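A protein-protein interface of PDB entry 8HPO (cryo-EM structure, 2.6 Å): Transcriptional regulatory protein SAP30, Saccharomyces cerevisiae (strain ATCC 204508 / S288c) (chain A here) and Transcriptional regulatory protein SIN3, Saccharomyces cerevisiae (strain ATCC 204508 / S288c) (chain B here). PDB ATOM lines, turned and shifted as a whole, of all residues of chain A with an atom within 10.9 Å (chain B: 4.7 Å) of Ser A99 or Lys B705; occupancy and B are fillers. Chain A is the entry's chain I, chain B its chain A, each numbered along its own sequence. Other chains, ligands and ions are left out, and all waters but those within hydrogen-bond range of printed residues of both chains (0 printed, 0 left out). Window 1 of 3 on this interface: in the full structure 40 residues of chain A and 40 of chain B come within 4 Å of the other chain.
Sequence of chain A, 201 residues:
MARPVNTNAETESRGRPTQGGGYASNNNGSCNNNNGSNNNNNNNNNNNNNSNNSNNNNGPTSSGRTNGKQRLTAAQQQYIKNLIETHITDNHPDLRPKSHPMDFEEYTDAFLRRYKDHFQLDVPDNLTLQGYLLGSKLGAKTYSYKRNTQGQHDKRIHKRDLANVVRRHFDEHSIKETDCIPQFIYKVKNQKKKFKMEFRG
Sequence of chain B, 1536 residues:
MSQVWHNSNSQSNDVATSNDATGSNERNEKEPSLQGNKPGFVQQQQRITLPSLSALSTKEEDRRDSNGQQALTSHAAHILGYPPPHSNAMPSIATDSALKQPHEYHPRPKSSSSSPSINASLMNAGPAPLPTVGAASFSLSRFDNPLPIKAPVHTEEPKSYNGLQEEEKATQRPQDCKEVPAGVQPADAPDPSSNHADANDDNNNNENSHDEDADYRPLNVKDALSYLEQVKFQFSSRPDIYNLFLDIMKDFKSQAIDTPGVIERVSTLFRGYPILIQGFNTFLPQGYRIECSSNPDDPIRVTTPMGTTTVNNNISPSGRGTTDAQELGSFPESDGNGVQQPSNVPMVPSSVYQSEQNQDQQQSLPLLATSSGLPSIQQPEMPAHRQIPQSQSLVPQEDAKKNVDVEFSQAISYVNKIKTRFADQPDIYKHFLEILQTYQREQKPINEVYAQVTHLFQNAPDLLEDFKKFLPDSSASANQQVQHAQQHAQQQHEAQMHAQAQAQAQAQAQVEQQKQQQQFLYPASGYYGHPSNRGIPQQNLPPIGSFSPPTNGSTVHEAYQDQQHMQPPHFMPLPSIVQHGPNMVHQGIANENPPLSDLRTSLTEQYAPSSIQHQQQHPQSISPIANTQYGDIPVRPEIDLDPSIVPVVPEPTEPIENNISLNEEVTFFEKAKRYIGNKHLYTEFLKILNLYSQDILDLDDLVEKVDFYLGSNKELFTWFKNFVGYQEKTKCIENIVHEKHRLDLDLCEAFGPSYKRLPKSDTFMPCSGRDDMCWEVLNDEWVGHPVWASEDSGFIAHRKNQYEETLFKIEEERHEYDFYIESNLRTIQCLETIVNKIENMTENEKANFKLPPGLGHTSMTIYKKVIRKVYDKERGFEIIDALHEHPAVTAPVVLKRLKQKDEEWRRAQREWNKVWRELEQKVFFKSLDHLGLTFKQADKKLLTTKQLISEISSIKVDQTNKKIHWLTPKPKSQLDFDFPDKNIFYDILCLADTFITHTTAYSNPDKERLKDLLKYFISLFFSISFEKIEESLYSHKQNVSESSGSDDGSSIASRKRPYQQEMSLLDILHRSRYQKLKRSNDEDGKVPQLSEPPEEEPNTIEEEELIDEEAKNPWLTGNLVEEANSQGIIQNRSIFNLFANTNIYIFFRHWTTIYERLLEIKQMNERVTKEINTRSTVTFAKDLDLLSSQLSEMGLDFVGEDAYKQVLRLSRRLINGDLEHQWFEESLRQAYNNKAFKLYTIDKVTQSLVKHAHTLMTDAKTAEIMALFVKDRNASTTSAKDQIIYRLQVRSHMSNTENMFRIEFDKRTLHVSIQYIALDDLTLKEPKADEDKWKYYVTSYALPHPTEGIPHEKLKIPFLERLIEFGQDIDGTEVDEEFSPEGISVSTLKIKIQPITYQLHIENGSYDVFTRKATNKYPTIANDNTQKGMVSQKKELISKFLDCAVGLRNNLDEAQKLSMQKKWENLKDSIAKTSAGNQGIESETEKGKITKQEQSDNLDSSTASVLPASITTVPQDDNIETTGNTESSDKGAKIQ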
ATOM      1  N   LEU A  95      11.545  31.023 -20.307  1.00  0.00           N
ATOM      2  CA  LEU A  95      11.575  30.583 -21.693  1.00  0.00           C
ATOM      3  C   LEU A  95      11.983  29.130 -21.864  1.00  0.00           C
ATOM      4  O   LEU A  95      12.045  28.661 -23.006  1.00  0.00           O
ATOM      5  CB  LEU A  95      12.529  31.458 -22.519  1.00  0.00           C
ATOM      6  CG  LEU A  95      12.099  32.889 -22.836  1.00  0.00           C
ATOM      7  CD1 LEU A  95      12.744  33.360 -24.131  1.00  0.00           C
ATOM      8  CD2 LEU A  95      10.588  32.998 -22.925  1.00  0.00           C
ATOM      9  N   ARG A  96      12.280  28.417 -20.784  1.00  0.00           N
ATOM     10  CA  ARG A  96      12.650  27.013 -20.875  1.00  0.00           C
ATOM     11  C   ARG A  96      11.549  26.225 -21.579  1.00  0.00           C
ATOM     12  O   ARG A  96      10.389  26.271 -21.148  1.00  0.00           O
ATOM     13  CB  ARG A  96      12.891  26.454 -19.476  1.00  0.00           C
ATOM     14  CG  ARG A  96      13.168  24.967 -19.425  1.00  0.00           C
ATOM     15  CD  ARG A  96      13.356  24.518 -17.986  1.00  0.00           C
ATOM     16  NE  ARG A  96      14.141  25.483 -17.220  1.00  0.00           N
ATOM     17  CZ  ARG A  96      14.168  25.546 -15.893  1.00  0.00           C
ATOM     18  NH1 ARG A  96      13.449  24.698 -15.170  1.00  0.00           N
ATOM     19  NH2 ARG A  96      14.913  26.459 -15.287  1.00  0.00           N
ATOM     20  N   PRO A  97      11.860  25.507 -22.659  1.00  0.00           N
ATOM     21  CA  PRO A  97      10.802  24.841 -23.430  1.00  0.00           C
ATOM     22  C   PRO A  97      10.081  23.788 -22.604  1.00  0.00           C
ATOM     23  O   PRO A  97      10.695  22.874 -22.051  1.00  0.00           O
ATOM     24  CB  PRO A  97      11.561  24.215 -24.606  1.00  0.00           C
ATOM     25  CG  PRO A  97      12.965  24.092 -24.132  1.00  0.00           C
ATOM     26  CD  PRO A  97      13.197  25.257 -23.219  1.00  0.00           C
ATOM     27  N   LYS A  98       8.759  23.930 -22.527  1.00  0.00           N
ATOM     28  CA  LYS A  98       7.903  23.074 -21.713  1.00  0.00           C
ATOM     29  C   LYS A  98       7.110  22.159 -22.640  1.00  0.00           C
ATOM     30  O   LYS A  98       6.626  22.595 -23.690  1.00  0.00           O
ATOM     31  CB  LYS A  98       6.979  23.912 -20.834  1.00  0.00           C
ATOM     32  CG  LYS A  98       7.696  24.646 -19.709  1.00  0.00           C
ATOM     33  CD  LYS A  98       6.851  25.775 -19.142  1.00  0.00           C
ATOM     34  CE  LYS A  98       6.260  26.637 -20.247  1.00  0.00           C
ATOM     35  NZ  LYS A  98       6.709  28.052 -20.158  1.00  0.00           N
ATOM     36  N   SER A  99       6.984  20.895 -22.249  1.00  0.00           N
ATOM     37  CA  SER A  99       6.328  19.900 -23.080  1.00  0.00           C
ATOM     38  C   SER A  99       4.811  19.974 -22.932  1.00  0.00           C
ATOM     39  O   SER A  99       4.275  20.569 -21.995  1.00  0.00           O
ATOM     40  CB  SER A  99       6.822  18.503 -22.712  1.00  0.00           C
ATOM     41  OG  SER A  99       7.098  18.423 -21.324  1.00  0.00           O
ATOM     42  N   HIS A 100       4.120  19.351 -23.883  1.00  0.00           N
ATOM     43  CA  HIS A 100       2.671  19.255 -23.829  1.00  0.00           C
ATOM     44  C   HIS A 100       2.244  18.352 -22.673  1.00  0.00           C
ATOM     45  O   HIS A 100       2.977  17.441 -22.282  1.00  0.00           O
ATOM     46  CB  HIS A 100       2.133  18.704 -25.146  1.00  0.00           C
ATOM     47  CG  HIS A 100       0.700  19.041 -25.408  1.00  0.00           C
ATOM     48  ND1 HIS A 100       0.315  20.172 -26.096  1.00  0.00           N
ATOM     49  CD2 HIS A 100      -0.442  18.391 -25.086  1.00  0.00           C
ATOM     50  CE1 HIS A 100      -1.003  20.209 -26.177  1.00  0.00           C
ATOM     51  NE2 HIS A 100      -1.487  19.140 -25.571  1.00  0.00           N
ATOM     52  N   PRO A 101       1.065  18.592 -22.094  1.00  0.00           N
ATOM     53  CA  PRO A 101       0.583  17.707 -21.021  1.00  0.00           C
ATOM     54  C   PRO A 101       0.090  16.356 -21.511  1.00  0.00           C
ATOM     55  O   PRO A 101       0.037  15.413 -20.712  1.00  0.00           O
ATOM     56  CB  PRO A 101      -0.557  18.515 -20.386  1.00  0.00           C
ATOM     57  CG  PRO A 101      -0.315  19.923 -20.812  1.00  0.00           C
ATOM     58  CD  PRO A 101       0.269  19.826 -22.176  1.00  0.00           C
ATOM     59  N   MET A 102      -0.260  16.225 -22.790  1.00  0.00           N
ATOM     60  CA  MET A 102      -0.786  14.974 -23.315  1.00  0.00           C
ATOM     61  C   MET A 102       0.294  14.025 -23.805  1.00  0.00           C
ATOM     62  O   MET A 102       0.005  12.845 -24.030  1.00  0.00           O
ATOM     63  CB  MET A 102      -1.762  15.248 -24.461  1.00  0.00           C
ATOM     64  CG  MET A 102      -3.040  15.928 -24.027  1.00  0.00           C
ATOM     65  SD  MET A 102      -3.623  15.326 -22.437  1.00  0.00           S
ATOM     66  CE  MET A 102      -4.450  16.790 -21.837  1.00  0.00           C
ATOM     67  N   ASP A 103       1.520  14.502 -23.988  1.00  0.00           N
ATOM     68  CA  ASP A 103       2.628  13.653 -24.402  1.00  0.00           C
ATOM     69  C   ASP A 103       3.249  13.073 -23.139  1.00  0.00           C
ATOM     70  O   ASP A 103       3.982  13.764 -22.428  1.00  0.00           O
ATOM     71  CB  ASP A 103       3.643  14.454 -25.213  1.00  0.00           C
ATOM     72  CG  ASP A 103       4.836  13.628 -25.652  1.00  0.00           C
ATOM     73  OD1 ASP A 103       4.900  12.420 -25.337  1.00  0.00           O
ATOM     74  OD2 ASP A 103       5.724  14.195 -26.322  1.00  0.00           O
ATOM     75  N   PHE A 104       2.951  11.810 -22.854  1.00  0.00           N
ATOM     76  CA  PHE A 104       3.332  11.207 -21.588  1.00  0.00           C
ATOM     77  C   PHE A 104       4.746  10.651 -21.589  1.00  0.00           C
ATOM     78  O   PHE A 104       5.186  10.119 -20.566  1.00  0.00           O
ATOM     79  CB  PHE A 104       2.339  10.108 -21.203  1.00  0.00           C
ATOM     80  CG  PHE A 104       1.076  10.635 -20.599  1.00  0.00           C
ATOM     81  CD1 PHE A 104       0.892  10.627 -19.228  1.00  0.00           C
ATOM     82  CD2 PHE A 104       0.083  11.163 -21.398  1.00  0.00           C
ATOM     83  CE1 PHE A 104      -0.265  11.124 -18.674  1.00  0.00           C
ATOM     84  CE2 PHE A 104      -1.070  11.659 -20.849  1.00  0.00           C
ATOM     85  CZ  PHE A 104      -1.244  11.642 -19.485  1.00  0.00           C
ATOM     86  N   GLU A 105       5.471  10.767 -22.701  1.00  0.00           N
ATOM     87  CA  GLU A 105       6.858  10.323 -22.706  1.00  0.00           C
ATOM     88  C   GLU A 105       7.757  11.304 -21.966  1.00  0.00           C
ATOM     89  O   GLU A 105       8.866  10.942 -21.557  1.00  0.00           O
ATOM     90  CB  GLU A 105       7.336  10.125 -24.142  1.00  0.00           C
ATOM     91  CG  GLU A 105       7.963   8.769 -24.396  1.00  0.00           C
ATOM     92  CD  GLU A 105       8.753   8.721 -25.687  1.00  0.00           C
ATOM     93  OE1 GLU A 105       9.993   8.580 -25.622  1.00  0.00           O
ATOM     94  OE2 GLU A 105       8.137   8.820 -26.768  1.00  0.00           O
ATOM     95  N   GLU A 106       7.300  12.541 -21.783  1.00  0.00           N
ATOM     96  CA  GLU A 106       8.075  13.572 -21.097  1.00  0.00           C
ATOM     97  C   GLU A 106       7.684  13.628 -19.621  1.00  0.00           C
ATOM     98  O   GLU A 106       7.390  14.687 -19.073  1.00  0.00           O
ATOM     99  CB  GLU A 106       7.854  14.924 -21.765  1.00  0.00           C
ATOM    100  CG  GLU A 106       8.623  15.156 -23.055  1.00  0.00           C
ATOM    101  CD  GLU A 106       8.551  13.991 -24.011  1.00  0.00           C
ATOM    102  OE1 GLU A 106       9.592  13.639 -24.600  1.00  0.00           O
ATOM    103  OE2 GLU A 106       7.454  13.425 -24.177  1.00  0.00           O
ATOM    104  N   TYR A 107       7.688  12.469 -18.970  1.00  0.00           N
ATOM    105  CA  TYR A 107       7.147  12.382 -17.617  1.00  0.00           C
ATOM    106  C   TYR A 107       8.029  11.543 -16.694  1.00  0.00           C
ATOM    107  O   TYR A 107       7.556  10.644 -16.002  1.00  0.00           O
ATOM    108  CB  TYR A 107       5.727  11.827 -17.644  1.00  0.00           C
ATOM    109  CG  TYR A 107       4.630  12.861 -17.781  1.00  0.00           C
ATOM    110  CD1 TYR A 107       3.907  13.286 -16.682  1.00  0.00           C
ATOM    111  CD2 TYR A 107       4.293  13.379 -19.016  1.00  0.00           C
ATOM    112  CE1 TYR A 107       2.895  14.208 -16.808  1.00  0.00           C
ATOM    113  CE2 TYR A 107       3.285  14.300 -19.149  1.00  0.00           C
ATOM    114  CZ  TYR A 107       2.587  14.708 -18.046  1.00  0.00           C
ATOM    115  OH  TYR A 107       1.581  15.628 -18.184  1.00  0.00           O
ATOM    116  N   THR A 108       9.334  11.779 -16.720  1.00  0.00           N
ATOM    117  CA  THR A 108      10.213  11.403 -15.613  1.00  0.00           C
ATOM    118  C   THR A 108      10.350   9.893 -15.415  1.00  0.00           C
ATOM    119  O   THR A 108      11.184   9.441 -14.625  1.00  0.00           O
ATOM    120  CB  THR A 108       9.700  12.047 -14.317  1.00  0.00           C
ATOM    121  OG1 THR A 108       9.389  13.420 -14.567  1.00  0.00           O
ATOM    122  CG2 THR A 108      10.739  11.994 -13.214  1.00  0.00           C
ATOM    123  N   ASP A 109       9.534   9.111 -16.114  1.00  0.00           N
ATOM    124  CA  ASP A 109       9.550   7.650 -16.103  1.00  0.00           C
ATOM    125  C   ASP A 109       9.347   7.065 -14.711  1.00  0.00           C
ATOM    126  O   ASP A 109       9.325   5.843 -14.551  1.00  0.00           O
ATOM    127  CB  ASP A 109      10.825   7.111 -16.789  1.00  0.00           C
ATOM    128  CG  ASP A 109      12.024   6.868 -15.844  1.00  0.00           C
ATOM    129  OD1 ASP A 109      11.945   6.952 -14.603  1.00  0.00           O
ATOM    130  OD2 ASP A 109      13.104   6.565 -16.392  1.00  0.00           O
ATOM    131  N   PHE A 111       6.791   8.928 -12.813  1.00  0.00           N
ATOM    132  CA  PHE A 111       5.363   9.140 -12.969  1.00  0.00           C
ATOM    133  C   PHE A 111       4.732   7.992 -13.734  1.00  0.00           C
ATOM    134  O   PHE A 111       3.659   7.512 -13.363  1.00  0.00           O
ATOM    135  CB  PHE A 111       5.104  10.457 -13.689  1.00  0.00           C
ATOM    136  CG  PHE A 111       3.737  10.559 -14.284  1.00  0.00           C
ATOM    137  CD1 PHE A 111       3.493  10.129 -15.574  1.00  0.00           C
ATOM    138  CD2 PHE A 111       2.697  11.092 -13.558  1.00  0.00           C
ATOM    139  CE1 PHE A 111       2.242  10.221 -16.117  1.00  0.00           C
ATOM    140  CE2 PHE A 111       1.447  11.191 -14.102  1.00  0.00           C
ATOM    141  CZ  PHE A 111       1.221  10.754 -15.384  1.00  0.00           C
ATOM    142  N   LEU A 112       5.368   7.554 -14.822  1.00  0.00           N
ATOM    143  CA  LEU A 112       4.812   6.467 -15.622  1.00  0.00           C
ATOM    144  C   LEU A 112       4.715   5.186 -14.810  1.00  0.00           C
ATOM    145  O   LEU A 112       3.700   4.482 -14.855  1.00  0.00           O
ATOM    146  CB  LEU A 112       5.664   6.246 -16.866  1.00  0.00           C
ATOM    147  CG  LEU A 112       5.589   7.345 -17.915  1.00  0.00           C
ATOM    148  CD1 LEU A 112       6.436   6.991 -19.115  1.00  0.00           C
ATOM    149  CD2 LEU A 112       4.159   7.576 -18.319  1.00  0.00           C
ATOM    150  N   LYS A 159      10.456   3.063 -23.463  1.00  0.00           N
ATOM    151  CA  LYS A 159       9.570   4.015 -22.801  1.00  0.00           C
ATOM    152  C   LYS A 159       8.364   4.391 -23.647  1.00  0.00           C
ATOM    153  O   LYS A 159       7.314   4.726 -23.088  1.00  0.00           O
ATOM    154  CB  LYS A 159      10.339   5.280 -22.436  1.00  0.00           C
ATOM    155  CG  LYS A 159      10.586   5.450 -20.957  1.00  0.00           C
ATOM    156  CD  LYS A 159      10.866   6.897 -20.596  1.00  0.00           C
ATOM    157  CE  LYS A 159       9.807   7.825 -21.152  1.00  0.00           C
ATOM    158  NZ  LYS A 159       9.964   9.203 -20.630  1.00  0.00           N
ATOM    159  N   PHE A 170      -5.392   6.646 -19.974  1.00  0.00           N
ATOM    160  CA  PHE A 170      -5.736   7.982 -19.513  1.00  0.00           C
ATOM    161  C   PHE A 170      -6.889   8.554 -20.319  1.00  0.00           C
ATOM    162  O   PHE A 170      -7.808   9.147 -19.749  1.00  0.00           O
ATOM    163  CB  PHE A 170      -4.504   8.882 -19.594  1.00  0.00           C
ATOM    164  CG  PHE A 170      -4.749  10.310 -19.201  1.00  0.00           C
ATOM    165  CD1 PHE A 170      -5.102  11.248 -20.146  1.00  0.00           C
ATOM    166  CD2 PHE A 170      -4.589  10.713 -17.894  1.00  0.00           C
ATOM    167  CE1 PHE A 170      -5.317  12.554 -19.790  1.00  0.00           C
ATOM    168  CE2 PHE A 170      -4.801  12.019 -17.533  1.00  0.00           C
ATOM    169  CZ  PHE A 170      -5.163  12.943 -18.483  1.00  0.00           C
ATOM    170  N   ILE B 688      -6.038  16.074 -14.896  1.00  0.00           N
ATOM    171  CA  ILE B 688      -4.671  16.259 -14.404  1.00  0.00           C
ATOM    172  C   ILE B 688      -4.676  16.662 -12.930  1.00  0.00           C
ATOM    173  O   ILE B 688      -3.829  16.216 -12.142  1.00  0.00           O
ATOM    174  CB  ILE B 688      -3.916  17.283 -15.265  1.00  0.00           C
ATOM    175  CG1 ILE B 688      -3.884  16.833 -16.721  1.00  0.00           C
ATOM    176  CG2 ILE B 688      -2.498  17.451 -14.756  1.00  0.00           C
ATOM    177  CD1 ILE B 688      -3.449  17.911 -17.664  1.00  0.00           C
ATOM    178  N   ASP B 701       5.767  19.356 -10.804  1.00  0.00           N
ATOM    179  CA  ASP B 701       5.302  18.952 -12.122  1.00  0.00           C
ATOM    180  C   ASP B 701       3.813  19.221 -12.281  1.00  0.00           C
ATOM    181  O   ASP B 701       3.342  19.441 -13.400  1.00  0.00           O
ATOM    182  CB  ASP B 701       5.617  17.479 -12.361  1.00  0.00           C
ATOM    183  CG  ASP B 701       5.668  17.128 -13.834  1.00  0.00           C
ATOM    184  OD1 ASP B 701       4.734  17.490 -14.573  1.00  0.00           O
ATOM    185  OD2 ASP B 701       6.647  16.479 -14.255  1.00  0.00           O
ATOM    186  N   LEU B 702       3.068  19.270 -11.176  1.00  0.00           N
ATOM    187  CA  LEU B 702       1.669  19.668 -11.271  1.00  0.00           C
ATOM    188  C   LEU B 702       1.545  21.102 -11.761  1.00  0.00           C
ATOM    189  O   LEU B 702       0.823  21.375 -12.726  1.00  0.00           O
ATOM    190  CB  LEU B 702       0.965  19.502  -9.927  1.00  0.00           C
ATOM    191  CG  LEU B 702      -0.408  20.182  -9.880  1.00  0.00           C
ATOM    192  CD1 LEU B 702      -1.365  19.621 -10.918  1.00  0.00           C
ATOM    193  CD2 LEU B 702      -1.011  20.107  -8.493  1.00  0.00           C
ATOM    194  N   VAL B 703       2.225  22.039 -11.096  1.00  0.00           N
ATOM    195  CA  VAL B 703       2.157  23.432 -11.541  1.00  0.00           C
ATOM    196  C   VAL B 703       2.705  23.565 -12.957  1.00  0.00           C
ATOM    197  O   VAL B 703       2.163  24.311 -13.788  1.00  0.00           O
ATOM    198  CB  VAL B 703       2.901  24.351 -10.555  1.00  0.00           C
ATOM    199  CG1 VAL B 703       2.460  25.783 -10.751  1.00  0.00           C
ATOM    200  CG2 VAL B 703       2.644  23.919  -9.129  1.00  0.00           C
ATOM    201  N   GLU B 704       3.778  22.830 -13.258  1.00  0.00           N
ATOM    202  CA  GLU B 704       4.340  22.826 -14.604  1.00  0.00           C
ATOM    203  C   GLU B 704       3.294  22.439 -15.643  1.00  0.00           C
ATOM    204  O   GLU B 704       3.168  23.096 -16.681  1.00  0.00           O
ATOM    205  CB  GLU B 704       5.535  21.874 -14.646  1.00  0.00           C
ATOM    206  CG  GLU B 704       6.589  22.189 -15.692  1.00  0.00           C
ATOM    207  CD  GLU B 704       6.087  22.032 -17.109  1.00  0.00           C
ATOM    208  OE1 GLU B 704       5.633  23.036 -17.695  1.00  0.00           O
ATOM    209  OE2 GLU B 704       6.140  20.902 -17.637  1.00  0.00           O
ATOM    210  N   LYS B 705       2.525  21.381 -15.381  1.00  0.00           N
ATOM    211  CA  LYS B 705       1.545  20.925 -16.363  1.00  0.00           C
ATOM    212  C   LYS B 705       0.321  21.830 -16.397  1.00  0.00           C
ATOM    213  O   LYS B 705      -0.335  21.953 -17.436  1.00  0.00           O
ATOM    214  CB  LYS B 705       1.139  19.483 -16.068  1.00  0.00           C
ATOM    215  CG  LYS B 705       2.271  18.496 -16.241  1.00  0.00           C
ATOM    216  CD  LYS B 705       2.841  18.562 -17.640  1.00  0.00           C
ATOM    217  CE  LYS B 705       4.180  17.857 -17.725  1.00  0.00           C
ATOM    218  NZ  LYS B 705       4.738  17.911 -19.107  1.00  0.00           N
ATOM    219  N   VAL B 706      -0.001  22.469 -15.271  1.00  0.00           N
ATOM    220  CA  VAL B 706      -1.115  23.412 -15.231  1.00  0.00           C
ATOM    221  C   VAL B 706      -0.795  24.654 -16.051  1.00  0.00           C
ATOM    222  O   VAL B 706      -1.704  25.311 -16.579  1.00  0.00           O
ATOM    223  CB  VAL B 706      -1.453  23.757 -13.768  1.00  0.00           C
ATOM    224  CG1 VAL B 706      -2.376  24.962 -13.684  1.00  0.00           C
ATOM    225  CG2 VAL B 706      -2.073  22.562 -13.079  1.00  0.00           C
ATOM    226  N   ASP B 707       0.497  24.994 -16.171  1.00  0.00           N
ATOM    227  CA  ASP B 707       0.914  26.135 -16.991  1.00  0.00           C
ATOM    228  C   ASP B 707       0.159  26.224 -18.310  1.00  0.00           C
ATOM    229  O   ASP B 707      -0.220  27.320 -18.734  1.00  0.00           O
ATOM    230  CB  ASP B 707       2.412  26.065 -17.303  1.00  0.00           C
ATOM    231  CG  ASP B 707       3.277  26.082 -16.064  1.00  0.00           C
ATOM    232  OD1 ASP B 707       4.432  25.616 -16.135  1.00  0.00           O
ATOM    233  OD2 ASP B 707       2.818  26.577 -15.022  1.00  0.00           O
ATOM    234  N   PHE B 708      -0.071  25.089 -18.971  1.00  0.00           N
ATOM    235  CA  PHE B 708      -0.661  25.124 -20.304  1.00  0.00           C
ATOM    236  C   PHE B 708      -2.129  25.531 -20.270  1.00  0.00           C
ATOM    237  O   PHE B 708      -2.712  25.824 -21.320  1.00  0.00           O
ATOM    238  CB  PHE B 708      -0.502  23.765 -20.982  1.00  0.00           C
ATOM    239  CG  PHE B 708      -0.972  23.742 -22.402  1.00  0.00           C
ATOM    240  CD1 PHE B 708      -1.769  22.714 -22.867  1.00  0.00           C
ATOM    241  CD2 PHE B 708      -0.621  24.757 -23.274  1.00  0.00           C
ATOM    242  CE1 PHE B 708      -2.208  22.696 -24.175  1.00  0.00           C
ATOM    243  CE2 PHE B 708      -1.056  24.742 -24.585  1.00  0.00           C
ATOM    244  CZ  PHE B 708      -1.850  23.709 -25.035  1.00  0.00           C
ATOM    245  N   TYR B 709      -2.744  25.562 -19.090  1.00  0.00           N
ATOM    246  CA  TYR B 709      -4.135  25.979 -18.975  1.00  0.00           C
ATOM    247  C   TYR B 709      -4.310  27.290 -18.226  1.00  0.00           C
ATOM    248  O   TYR B 709      -5.236  28.046 -18.535  1.00  0.00           O
ATOM    249  CB  TYR B 709      -4.964  24.892 -18.279  1.00  0.00           C
ATOM    250  CG  TYR B 709      -4.759  23.504 -18.841  1.00  0.00           C
ATOM    251  CD1 TYR B 709      -5.278  23.152 -20.079  1.00  0.00           C
ATOM    252  CD2 TYR B 709      -4.056  22.547 -18.131  1.00  0.00           C
ATOM    253  CE1 TYR B 709      -5.091  21.889 -20.595  1.00  0.00           C
ATOM    254  CE2 TYR B 709      -3.864  21.281 -18.640  1.00  0.00           C
ATOM    255  CZ  TYR B 709      -4.381  20.958 -19.871  1.00  0.00           C
ATOM    256  OH  TYR B 709      -4.191  19.695 -20.374  1.00  0.00           O
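OG of Ser A99 sits at hydrogen-bond distance from NZ of Lys B705, 3.3 Å away.
The side-chain hydroxyl (OH) of Tyr A107 lies within hydrogen-bond range of the backbone carbonyl oxygen (O) of Pro A101, 3.0 Å away. The backbone carbonyl oxygen (O) of Val B703 sits close to the side-chain carboxylate (OD2) of Asp B707 (2.7 Å). The side-chain carboxylate (OE2) of Glu B704 lies within salt-bridge range of the side-chain amino group (NZ) of Lys B705 (3.6 Å).
Among the printed residues, merely in contact across the chains: Lys A98 with Glu B704 (3.3 Å), Lys A98 with Asp B707 (3.9 Å), His A100 with Lys B705 (3.7 Å), His A100 with Phe B708 (3.4 Å), Pro A101 with Lys B705 (3.9 Å), Pro A101 with Phe B708 (3.6 Å), Pro A101 with Tyr B709 (3.8 Å), Met A102 with Tyr B709 (3.3 Å) and Tyr A107 with Lys B705 (3.2 Å).
Of chain B, only Lys B705 (3.3 Å) comes within 4 Å of Ser A99. Of chain A, only Ser A99, His A100, Pro A101 and Tyr A107 come within 4 Å of Lys B705. No residue of chain A comes within 4 Å of Val B703. No residue of chain A comes within 4 Å of Val B706. Of the printed residues of chain A, Asp B707 touches Lys A98. Of the printed residues of chain B, Tyr A107 touches Lys B705 (3.2 Å). Printed residues of chain A within 4 Å of Phe B708: His A100 (3.4 Å) and Pro A101 (3.6 Å). Of the printed residues of chain B, His A100 touches Lys B705 and Phe B708. Of the printed residues of chain A, Tyr B709 touches Pro A101 (3.8 Å) and Met A102 (3.3 Å). Leu A112 touches none of the printed residues of chain B. Phe A111 touches none of the printed residues of chain B. The nearest residue of chain B that does not touch Ser A99 is Glu B704 (4.5 Å). The nearest printed residue of chain B that does not touch Met A102 is Ile B688 (4.4 Å).
Of the 10 printed residues of chain B, 5 touch a printed residue of chain A. Printed residues of chain B that touch a printed residue of chain A: Glu B704, Lys B705, Asp B707, Phe B708 and Tyr B709. Hydrophobic or aromatic side chains of chain A that line the printed part of chain B: His A100, Pro A101, Met A102 and Tyr A107. Among the printed residues, 10 pairs touch across the chains. Among the printed residues, no Asp or Glu carboxylate lies within 4 Å of a Lys or Arg side-chain nitrogen of the other chain.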
